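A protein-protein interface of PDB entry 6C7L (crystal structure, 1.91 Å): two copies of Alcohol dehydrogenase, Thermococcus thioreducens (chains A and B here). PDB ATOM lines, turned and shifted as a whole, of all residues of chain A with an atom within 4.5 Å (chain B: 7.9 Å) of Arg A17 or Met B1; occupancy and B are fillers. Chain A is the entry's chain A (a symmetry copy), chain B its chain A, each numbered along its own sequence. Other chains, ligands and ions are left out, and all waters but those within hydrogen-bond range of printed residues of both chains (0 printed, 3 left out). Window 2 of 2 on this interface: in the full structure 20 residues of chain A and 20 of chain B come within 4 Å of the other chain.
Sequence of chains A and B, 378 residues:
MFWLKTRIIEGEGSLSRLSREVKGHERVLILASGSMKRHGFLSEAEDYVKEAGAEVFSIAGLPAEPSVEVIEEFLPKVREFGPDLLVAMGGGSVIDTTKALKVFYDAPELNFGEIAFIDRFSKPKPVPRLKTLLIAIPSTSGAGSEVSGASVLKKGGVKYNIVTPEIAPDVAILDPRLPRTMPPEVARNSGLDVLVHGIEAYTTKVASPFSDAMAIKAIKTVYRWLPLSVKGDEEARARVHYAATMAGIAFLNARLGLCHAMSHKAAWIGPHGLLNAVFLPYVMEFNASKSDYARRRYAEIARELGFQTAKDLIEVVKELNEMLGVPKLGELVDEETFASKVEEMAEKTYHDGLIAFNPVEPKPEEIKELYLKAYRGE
Of the printed residues of chain B, Arg A17 touches Met B1 (3.0 Å). Of the printed residues of chain A, Met B1 touches Arg A7, Ile A8, Glu A10 and Arg A17. No residue of chain B comes within 4 Å of Ser A16. Of the printed residues of chain B, Glu A10 touches Met B1 and Ser B208. Of the printed residues of chain A, Ser B208 touches Glu A10 (3.4 Å). Ala B207 touches none of the printed residues of chain A. The nearest printed residue of chain B that does not touch Arg A17 is Phe B2 (7.5 Å). The nearest printed residue of chain A that does not touch Met B1 is Ile A9 (4.1 Å).
The backbone NH of Phe B2 is in hydrogen-bond range of the backbone carbonyl oxygen of Ile A8. The side-chain sulfur of Met B1 sits at hydrogen-bond distance from the guanidinium group of Arg A7, at 3.3 Å. NH2 of Arg A17 is in hydrogen-bond range of SD of Met B1.
The side-chain hydroxyl (OG) of Ser B208 lies close to the backbone NH (N) of Phe B210, at 3.2 Å. The backbone NH (N) of Ser B208 sits at hydrogen-bond distance from the side-chain hydroxyl (OG) of Ser B211 (3.0 Å). The side-chain carboxylate of Glu A21 lies within salt-bridge range of the guanidinium group of Arg A17 (2.9 Å). The guanidinium group (NH2) of Arg A7 lies within salt-bridge range of the side-chain carboxylate (OE1) of Glu A21 (2.8 Å).
No position is printed for both chains. Of the 7 pairs that touch across the chains among the printed residues, none has its exchanged pair printed and touching as well.
Arg A7 touches Phe B2 (CA to O, 3.7 Å). O of Ile A8 touches CA of Met B1, at 3.1 Å. Glu A10 touches Met B1. Glu A10 touches Ser B208.
Of the 12 printed residues of chain A, 4 touch a printed residue of chain B. Printed residues of chain A that touch a printed residue of chain B: Arg A7, Ile A8, Glu A10 and Arg A17. Among the printed residues, 7 pairs touch across the chains. Among the printed residues, no Asp or Glu carboxylate lies within 4 Å of a Lys or Arg side-chain nitrogen of the other chain.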
ATOM      1  N   ARG A   7       3.200 -19.877  13.622  1.00  0.00           N
ATOM      2  CA  ARG A   7       2.587 -20.778  14.591  1.00  0.00           C
ATOM      3  C   ARG A   7       1.737 -21.819  13.868  1.00  0.00           C
ATOM      4  O   ARG A   7       0.897 -21.465  13.027  1.00  0.00           O
ATOM      5  CB  ARG A   7       1.716 -19.968  15.564  1.00  0.00           C
ATOM      6  CG  ARG A   7       0.987 -20.817  16.586  1.00  0.00           C
ATOM      7  CD  ARG A   7       0.604 -20.004  17.816  1.00  0.00           C
ATOM      8  NE  ARG A   7      -0.054 -18.758  17.442  1.00  0.00           N
ATOM      9  CZ  ARG A   7      -1.333 -18.656  17.096  1.00  0.00           C
ATOM     10  NH1 ARG A   7      -2.133 -19.703  17.211  1.00  0.00           N
ATOM     11  NH2 ARG A   7      -1.836 -17.473  16.755  1.00  0.00           N
ATOM     12  N   ILE A   8       1.990 -23.089  14.157  1.00  0.00           N
ATOM     13  CA  ILE A   8       1.363 -24.180  13.435  1.00  0.00           C
ATOM     14  C   ILE A   8       0.245 -24.832  14.262  1.00  0.00           C
ATOM     15  O   ILE A   8       0.435 -25.249  15.420  1.00  0.00           O
ATOM     16  CB  ILE A   8       2.397 -25.228  13.028  1.00  0.00           C
ATOM     17  CG1 ILE A   8       3.453 -24.581  12.138  1.00  0.00           C
ATOM     18  CG2 ILE A   8       1.734 -26.377  12.288  1.00  0.00           C
ATOM     19  CD1 ILE A   8       4.651 -25.468  11.934  1.00  0.00           C
ATOM     20  N   ILE A   9      -0.942 -24.805  13.686  1.00  0.00           N
ATOM     21  CA  ILE A   9      -2.096 -25.530  14.213  1.00  0.00           C
ATOM     22  C   ILE A   9      -2.336 -26.747  13.341  1.00  0.00           C
ATOM     23  O   ILE A   9      -2.373 -26.622  12.118  1.00  0.00           O
ATOM     24  CB  ILE A   9      -3.339 -24.621  14.191  1.00  0.00           C
ATOM     25  CG1 ILE A   9      -3.151 -23.411  15.113  1.00  0.00           C
ATOM     26  CG2 ILE A   9      -4.586 -25.391  14.601  1.00  0.00           C
ATOM     27  CD1 ILE A   9      -4.142 -22.309  14.809  1.00  0.00           C
ATOM     28  N   GLU A  10      -2.430 -27.928  13.946  1.00  0.00           N
ATOM     29  CA  GLU A  10      -2.485 -29.181  13.192  1.00  0.00           C
ATOM     30  C   GLU A  10      -3.419 -30.161  13.876  1.00  0.00           C
ATOM     31  O   GLU A  10      -3.521 -30.183  15.093  1.00  0.00           O
ATOM     32  CB  GLU A  10      -1.083 -29.784  13.017  1.00  0.00           C
ATOM     33  CG  GLU A  10      -0.590 -30.682  14.154  1.00  0.00           C
ATOM     34  CD  GLU A  10      -0.165 -29.903  15.384  1.00  0.00           C
ATOM     35  OE1 GLU A  10       0.262 -28.732  15.243  1.00  0.00           O
ATOM     36  OE2 GLU A  10      -0.240 -30.465  16.491  1.00  0.00           O
ATOM     37  N   SER A  14      -9.141 -29.314  12.560  1.00  0.00           N
ATOM     38  CA  SER A  14      -8.467 -28.093  12.984  1.00  0.00           C
ATOM     39  C   SER A  14      -8.799 -26.860  12.131  1.00  0.00           C
ATOM     40  O   SER A  14      -8.586 -25.740  12.587  1.00  0.00           O
ATOM     41  CB  SER A  14      -6.937 -28.304  13.071  1.00  0.00           C
ATOM     42  OG  SER A  14      -6.383 -28.492  11.784  1.00  0.00           O
ATOM     43  N   LEU A  15      -9.455 -27.031  10.982  1.00  0.00           N
ATOM     44  CA  LEU A  15      -9.992 -25.862  10.264  1.00  0.00           C
ATOM     45  C   LEU A  15     -10.889 -24.965  11.143  1.00  0.00           C
ATOM     46  O   LEU A  15     -10.923 -23.740  10.970  1.00  0.00           O
ATOM     47  CB  LEU A  15     -10.752 -26.270   8.989  1.00  0.00           C
ATOM     48  CG  LEU A  15     -11.156 -25.104   8.079  1.00  0.00           C
ATOM     49  CD1 LEU A  15      -9.954 -24.286   7.626  1.00  0.00           C
ATOM     50  CD2 LEU A  15     -11.920 -25.578   6.865  1.00  0.00           C
ATOM     51  N   SER A  16     -11.651 -25.587  12.038  1.00  0.00           N
ATOM     52  CA  SER A  16     -12.521 -24.856  12.953  1.00  0.00           C
ATOM     53  C   SER A  16     -11.785 -23.919  13.921  1.00  0.00           C
ATOM     54  O   SER A  16     -12.390 -22.977  14.448  1.00  0.00           O
ATOM     55  CB  SER A  16     -13.412 -25.824  13.761  1.00  0.00           C
ATOM     56  OG  SER A  16     -12.684 -26.422  14.820  1.00  0.00           O
ATOM     57  N   ARG A  17     -10.487 -24.141  14.111  1.00  0.00           N
ATOM     58  CA  ARG A  17      -9.658 -23.230  14.905  1.00  0.00           C
ATOM     59  C   ARG A  17      -9.442 -21.863  14.264  1.00  0.00           C
ATOM     60  O   ARG A  17      -8.860 -20.983  14.886  1.00  0.00           O
ATOM     61  CB  ARG A  17      -8.299 -23.869  15.207  1.00  0.00           C
ATOM     62  CG  ARG A  17      -8.351 -24.858  16.363  1.00  0.00           C
ATOM     63  CD  ARG A  17      -8.143 -24.146  17.691  1.00  0.00           C
ATOM     64  NE  ARG A  17      -6.743 -24.185  18.093  1.00  0.00           N
ATOM     65  CZ  ARG A  17      -5.924 -23.135  18.121  1.00  0.00           C
ATOM     66  NH1 ARG A  17      -6.363 -21.914  17.845  1.00  0.00           N
ATOM     67  NH2 ARG A  17      -4.660 -23.310  18.476  1.00  0.00           N
ATOM     68  N   LEU A  18      -9.899 -21.693  13.026  1.00  0.00           N
ATOM     69  CA  LEU A  18      -9.985 -20.369  12.424  1.00  0.00           C
ATOM     70  C   LEU A  18     -10.826 -19.401  13.278  1.00  0.00           C
ATOM     71  O   LEU A  18     -10.491 -18.208  13.386  1.00  0.00           O
ATOM     72  CB  LEU A  18     -10.523 -20.471  10.996  1.00  0.00           C
ATOM     73  CG  LEU A  18     -10.418 -19.262  10.067  1.00  0.00           C
ATOM     74  CD1 LEU A  18      -9.005 -18.692  10.037  1.00  0.00           C
ATOM     75  CD2 LEU A  18     -10.854 -19.657   8.659  1.00  0.00           C
ATOM     76  N   SER A  19     -11.904 -19.890  13.896  1.00  0.00           N
ATOM     77  CA  SER A  19     -12.726 -19.000  14.742  1.00  0.00           C
ATOM     78  C   SER A  19     -11.897 -18.344  15.838  1.00  0.00           C
ATOM     79  O   SER A  19     -11.950 -17.130  16.009  1.00  0.00           O
ATOM     80  CB  SER A  19     -13.884 -19.743  15.378  1.00  0.00           C
ATOM     81  OG  SER A  19     -14.709 -20.308  14.375  1.00  0.00           O
ATOM     82  N   ARG A  20     -11.081 -19.150  16.519  1.00  0.00           N
ATOM     83  CA  ARG A  20     -10.218 -18.667  17.582  1.00  0.00           C
ATOM     84  C   ARG A  20      -9.178 -17.720  17.030  1.00  0.00           C
ATOM     85  O   ARG A  20      -8.927 -16.668  17.616  1.00  0.00           O
ATOM     86  CB  ARG A  20      -9.562 -19.844  18.290  1.00  0.00           C
ATOM     87  CG  ARG A  20      -8.734 -19.484  19.519  1.00  0.00           C
ATOM     88  CD  ARG A  20      -8.204 -20.733  20.236  1.00  0.00           C
ATOM     89  NE  ARG A  20      -8.977 -21.949  19.949  1.00  0.00           N
ATOM     90  CZ  ARG A  20      -9.132 -22.960  20.802  1.00  0.00           C
ATOM     91  NH1 ARG A  20      -8.547 -22.929  21.994  1.00  0.00           N
ATOM     92  NH2 ARG A  20      -9.865 -24.010  20.452  1.00  0.00           N
ATOM     93  N   GLU A  21      -8.637 -18.039  15.854  1.00  0.00           N
ATOM     94  CA  GLU A  21      -7.570 -17.238  15.273  1.00  0.00           C
ATOM     95  C   GLU A  21      -8.031 -15.897  14.722  1.00  0.00           C
ATOM     96  O   GLU A  21      -7.224 -14.990  14.569  1.00  0.00           O
ATOM     97  CB  GLU A  21      -6.845 -18.008  14.180  1.00  0.00           C
ATOM     98  CG  GLU A  21      -6.117 -19.235  14.676  1.00  0.00           C
ATOM     99  CD  GLU A  21      -5.037 -18.921  15.699  1.00  0.00           C
ATOM    100  OE1 GLU A  21      -4.353 -17.895  15.536  1.00  0.00           O
ATOM    101  OE2 GLU A  21      -4.928 -19.672  16.688  1.00  0.00           O
ATOM    102  N   MET B   1      -0.626 -27.020  19.379  1.00  0.00           N
ATOM    103  CA  MET B   1       0.066 -26.253  18.329  1.00  0.00           C
ATOM    104  C   MET B   1       1.558 -26.619  18.313  1.00  0.00           C
ATOM    105  O   MET B   1       2.052 -27.320  19.210  1.00  0.00           O
ATOM    106  CB  MET B   1      -0.091 -24.750  18.590  1.00  0.00           C
ATOM    107  CG  MET B   1      -1.500 -24.332  18.918  1.00  0.00           C
ATOM    108  SD  MET B   1      -1.753 -22.553  18.921  1.00  0.00           S
ATOM    109  CE  MET B   1      -2.597 -22.321  20.492  1.00  0.00           C
ATOM    110  N   PHE B   2       2.280 -25.991  17.395  1.00  0.00           N
ATOM    111  CA  PHE B   2       3.744 -25.943  17.455  1.00  0.00           C
ATOM    112  C   PHE B   2       4.184 -24.505  17.154  1.00  0.00           C
ATOM    113  O   PHE B   2       3.776 -23.924  16.153  1.00  0.00           O
ATOM    114  CB  PHE B   2       4.347 -26.928  16.439  1.00  0.00           C
ATOM    115  CG  PHE B   2       5.854 -26.989  16.473  1.00  0.00           C
ATOM    116  CD1 PHE B   2       6.518 -27.695  17.472  1.00  0.00           C
ATOM    117  CD2 PHE B   2       6.596 -26.214  15.625  1.00  0.00           C
ATOM    118  CE1 PHE B   2       7.891 -27.659  17.578  1.00  0.00           C
ATOM    119  CE2 PHE B   2       7.975 -26.185  15.709  1.00  0.00           C
ATOM    120  CZ  PHE B   2       8.626 -26.983  16.636  1.00  0.00           C
ATOM    121  N   TRP B   3       4.990 -23.935  18.028  1.00  0.00           N
ATOM    122  CA  TRP B   3       5.531 -22.609  17.807  1.00  0.00           C
ATOM    123  C   TRP B   3       6.889 -22.502  18.467  1.00  0.00           C
ATOM    124  O   TRP B   3       7.232 -23.272  19.381  1.00  0.00           O
ATOM    125  CB  TRP B   3       4.586 -21.525  18.349  1.00  0.00           C
ATOM    126  CG  TRP B   3       4.366 -21.627  19.802  1.00  0.00           C
ATOM    127  CD1 TRP B   3       3.561 -22.525  20.442  1.00  0.00           C
ATOM    128  CD2 TRP B   3       5.060 -20.905  20.832  1.00  0.00           C
ATOM    129  NE1 TRP B   3       3.699 -22.396  21.807  1.00  0.00           N
ATOM    130  CE2 TRP B   3       4.631 -21.427  22.071  1.00  0.00           C
ATOM    131  CE3 TRP B   3       6.010 -19.880  20.825  1.00  0.00           C
ATOM    132  CZ2 TRP B   3       5.076 -20.914  23.296  1.00  0.00           C
ATOM    133  CZ3 TRP B   3       6.494 -19.404  22.050  1.00  0.00           C
ATOM    134  CH2 TRP B   3       6.000 -19.895  23.261  1.00  0.00           C
ATOM    135  N   VAL B 206       0.041 -34.261  24.493  1.00  0.00           N
ATOM    136  CA  VAL B 206      -0.023 -33.187  23.508  1.00  0.00           C
ATOM    137  C   VAL B 206       1.173 -33.158  22.543  1.00  0.00           C
ATOM    138  O   VAL B 206       1.418 -32.155  21.870  1.00  0.00           O
ATOM    139  CB  VAL B 206      -0.176 -31.815  24.213  1.00  0.00           C
ATOM    140  CG1 VAL B 206      -1.518 -31.747  24.950  1.00  0.00           C
ATOM    141  CG2 VAL B 206       0.974 -31.561  25.195  1.00  0.00           C
ATOM    142  N   ALA B 207       1.924 -34.251  22.482  1.00  0.00           N
ATOM    143  CA  ALA B 207       3.034 -34.357  21.538  1.00  0.00           C
ATOM    144  C   ALA B 207       2.460 -34.197  20.129  1.00  0.00           C
ATOM    145  O   ALA B 207       1.320 -34.593  19.874  1.00  0.00           O
ATOM    146  CB  ALA B 207       3.702 -35.715  21.682  1.00  0.00           C
ATOM    147  N   SER B 208       3.174 -33.484  19.275  1.00  0.00           N
ATOM    148  CA  SER B 208       2.820 -33.392  17.873  1.00  0.00           C
ATOM    149  C   SER B 208       3.938 -34.005  17.039  1.00  0.00           C
ATOM    150  O   SER B 208       5.055 -34.212  17.526  1.00  0.00           O
ATOM    151  CB  SER B 208       2.618 -31.927  17.468  1.00  0.00           C
ATOM    152  OG  SER B 208       3.865 -31.249  17.459  1.00  0.00           O
ATOM    153  N   PRO B 209       3.692 -34.195  15.747  1.00  0.00           N
ATOM    154  CA  PRO B 209       4.807 -34.581  14.870  1.00  0.00           C
ATOM    155  C   PRO B 209       5.994 -33.605  14.907  1.00  0.00           C
ATOM    156  O   PRO B 209       7.143 -34.027  14.753  1.00  0.00           O
ATOM    157  CB  PRO B 209       4.160 -34.584  13.477  1.00  0.00           C
ATOM    158  CG  PRO B 209       2.730 -34.870  13.741  1.00  0.00           C
ATOM    159  CD  PRO B 209       2.409 -34.162  15.031  1.00  0.00           C
ATOM    160  N   PHE B 210       5.701 -32.304  15.080  1.00  0.00           N
ATOM    161  CA  PHE B 210       6.700 -31.262  15.022  1.00  0.00           C
ATOM    162  C   PHE B 210       7.575 -31.285  16.286  1.00  0.00           C
ATOM    163  O   PHE B 210       8.794 -31.195  16.206  1.00  0.00           O
ATOM    164  CB  PHE B 210       6.004 -29.887  14.820  1.00  0.00           C
ATOM    165  CG  PHE B 210       5.188 -29.808  13.572  1.00  0.00           C
ATOM    166  CD1 PHE B 210       5.805 -29.624  12.348  1.00  0.00           C
ATOM    167  CD2 PHE B 210       3.843 -30.110  13.578  1.00  0.00           C
ATOM    168  CE1 PHE B 210       5.074 -29.600  11.170  1.00  0.00           C
ATOM    169  CE2 PHE B 210       3.120 -30.169  12.406  1.00  0.00           C
ATOM    170  CZ  PHE B 210       3.731 -29.885  11.194  1.00  0.00           C
ATOM    171  N   SER B 211       6.964 -31.454  17.454  1.00  0.00           N
ATOM    172  CA  SER B 211       7.737 -31.595  18.664  1.00  0.00           C
ATOM    173  C   SER B 211       8.504 -32.913  18.688  1.00  0.00           C
ATOM    174  O   SER B 211       9.641 -32.971  19.153  1.00  0.00           O
ATOM    175  CB  SER B 211       6.870 -31.438  19.920  1.00  0.00           C
ATOM    176  OG  SER B 211       5.839 -32.388  20.006  1.00  0.00           O
ATOM    177  N   ALA B 250      11.194 -29.217  21.947  1.00  0.00           N
ATOM    178  CA  ALA B 250      10.212 -30.256  22.123  1.00  0.00           C
ATOM    179  C   ALA B 250       9.319 -30.018  23.348  1.00  0.00           C
ATOM    180  O   ALA B 250       8.077 -30.081  23.240  1.00  0.00           O
ATOM    181  CB  ALA B 250      10.882 -31.614  22.181  1.00  0.00           C
ATOM    182  N   LEU B 252       8.937 -27.316  25.269  1.00  0.00           N
ATOM    183  CA  LEU B 252       8.225 -26.050  25.170  1.00  0.00           C
ATOM    184  C   LEU B 252       6.830 -26.310  24.601  1.00  0.00           C
ATOM    185  O   LEU B 252       5.850 -25.711  25.022  1.00  0.00           O
ATOM    186  CB  LEU B 252       8.967 -25.078  24.241  1.00  0.00           C
ATOM    187  CG  LEU B 252       8.183 -23.908  23.625  1.00  0.00           C
ATOM    188  CD1 LEU B 252       7.862 -22.852  24.676  1.00  0.00           C
ATOM    189  CD2 LEU B 252       8.979 -23.288  22.488  1.00  0.00           C
ATOM    190  N   ASN B 253       6.759 -27.202  23.624  1.00  0.00           N
ATOM    191  CA  ASN B 253       5.519 -27.447  22.923  1.00  0.00           C
ATOM    192  C   ASN B 253       4.717 -28.637  23.498  1.00  0.00           C
ATOM    193  O   ASN B 253       3.504 -28.543  23.743  1.00  0.00           O
ATOM    194  CB  ASN B 253       5.854 -27.664  21.439  1.00  0.00           C
ATOM    195  CG  ASN B 253       6.112 -26.369  20.720  1.00  0.00           C
ATOM    196  OD1 ASN B 253       5.173 -25.666  20.380  1.00  0.00           O
ATOM    197  ND2 ASN B 253       7.377 -25.967  20.638  1.00  0.00           N
ATOM    198  N   ALA B 254       5.412 -29.701  23.848  1.00  0.00           N
ATOM    199  CA  ALA B 254       4.763 -30.950  24.259  1.00  0.00           C
ATOM    200  C   ALA B 254       4.626 -31.090  25.796  1.00  0.00           C
ATOM    201  O   ALA B 254       3.952 -32.012  26.306  1.00  0.00           O
ATOM    202  CB  ALA B 254       5.542 -32.126  23.689  1.00  0.00           C
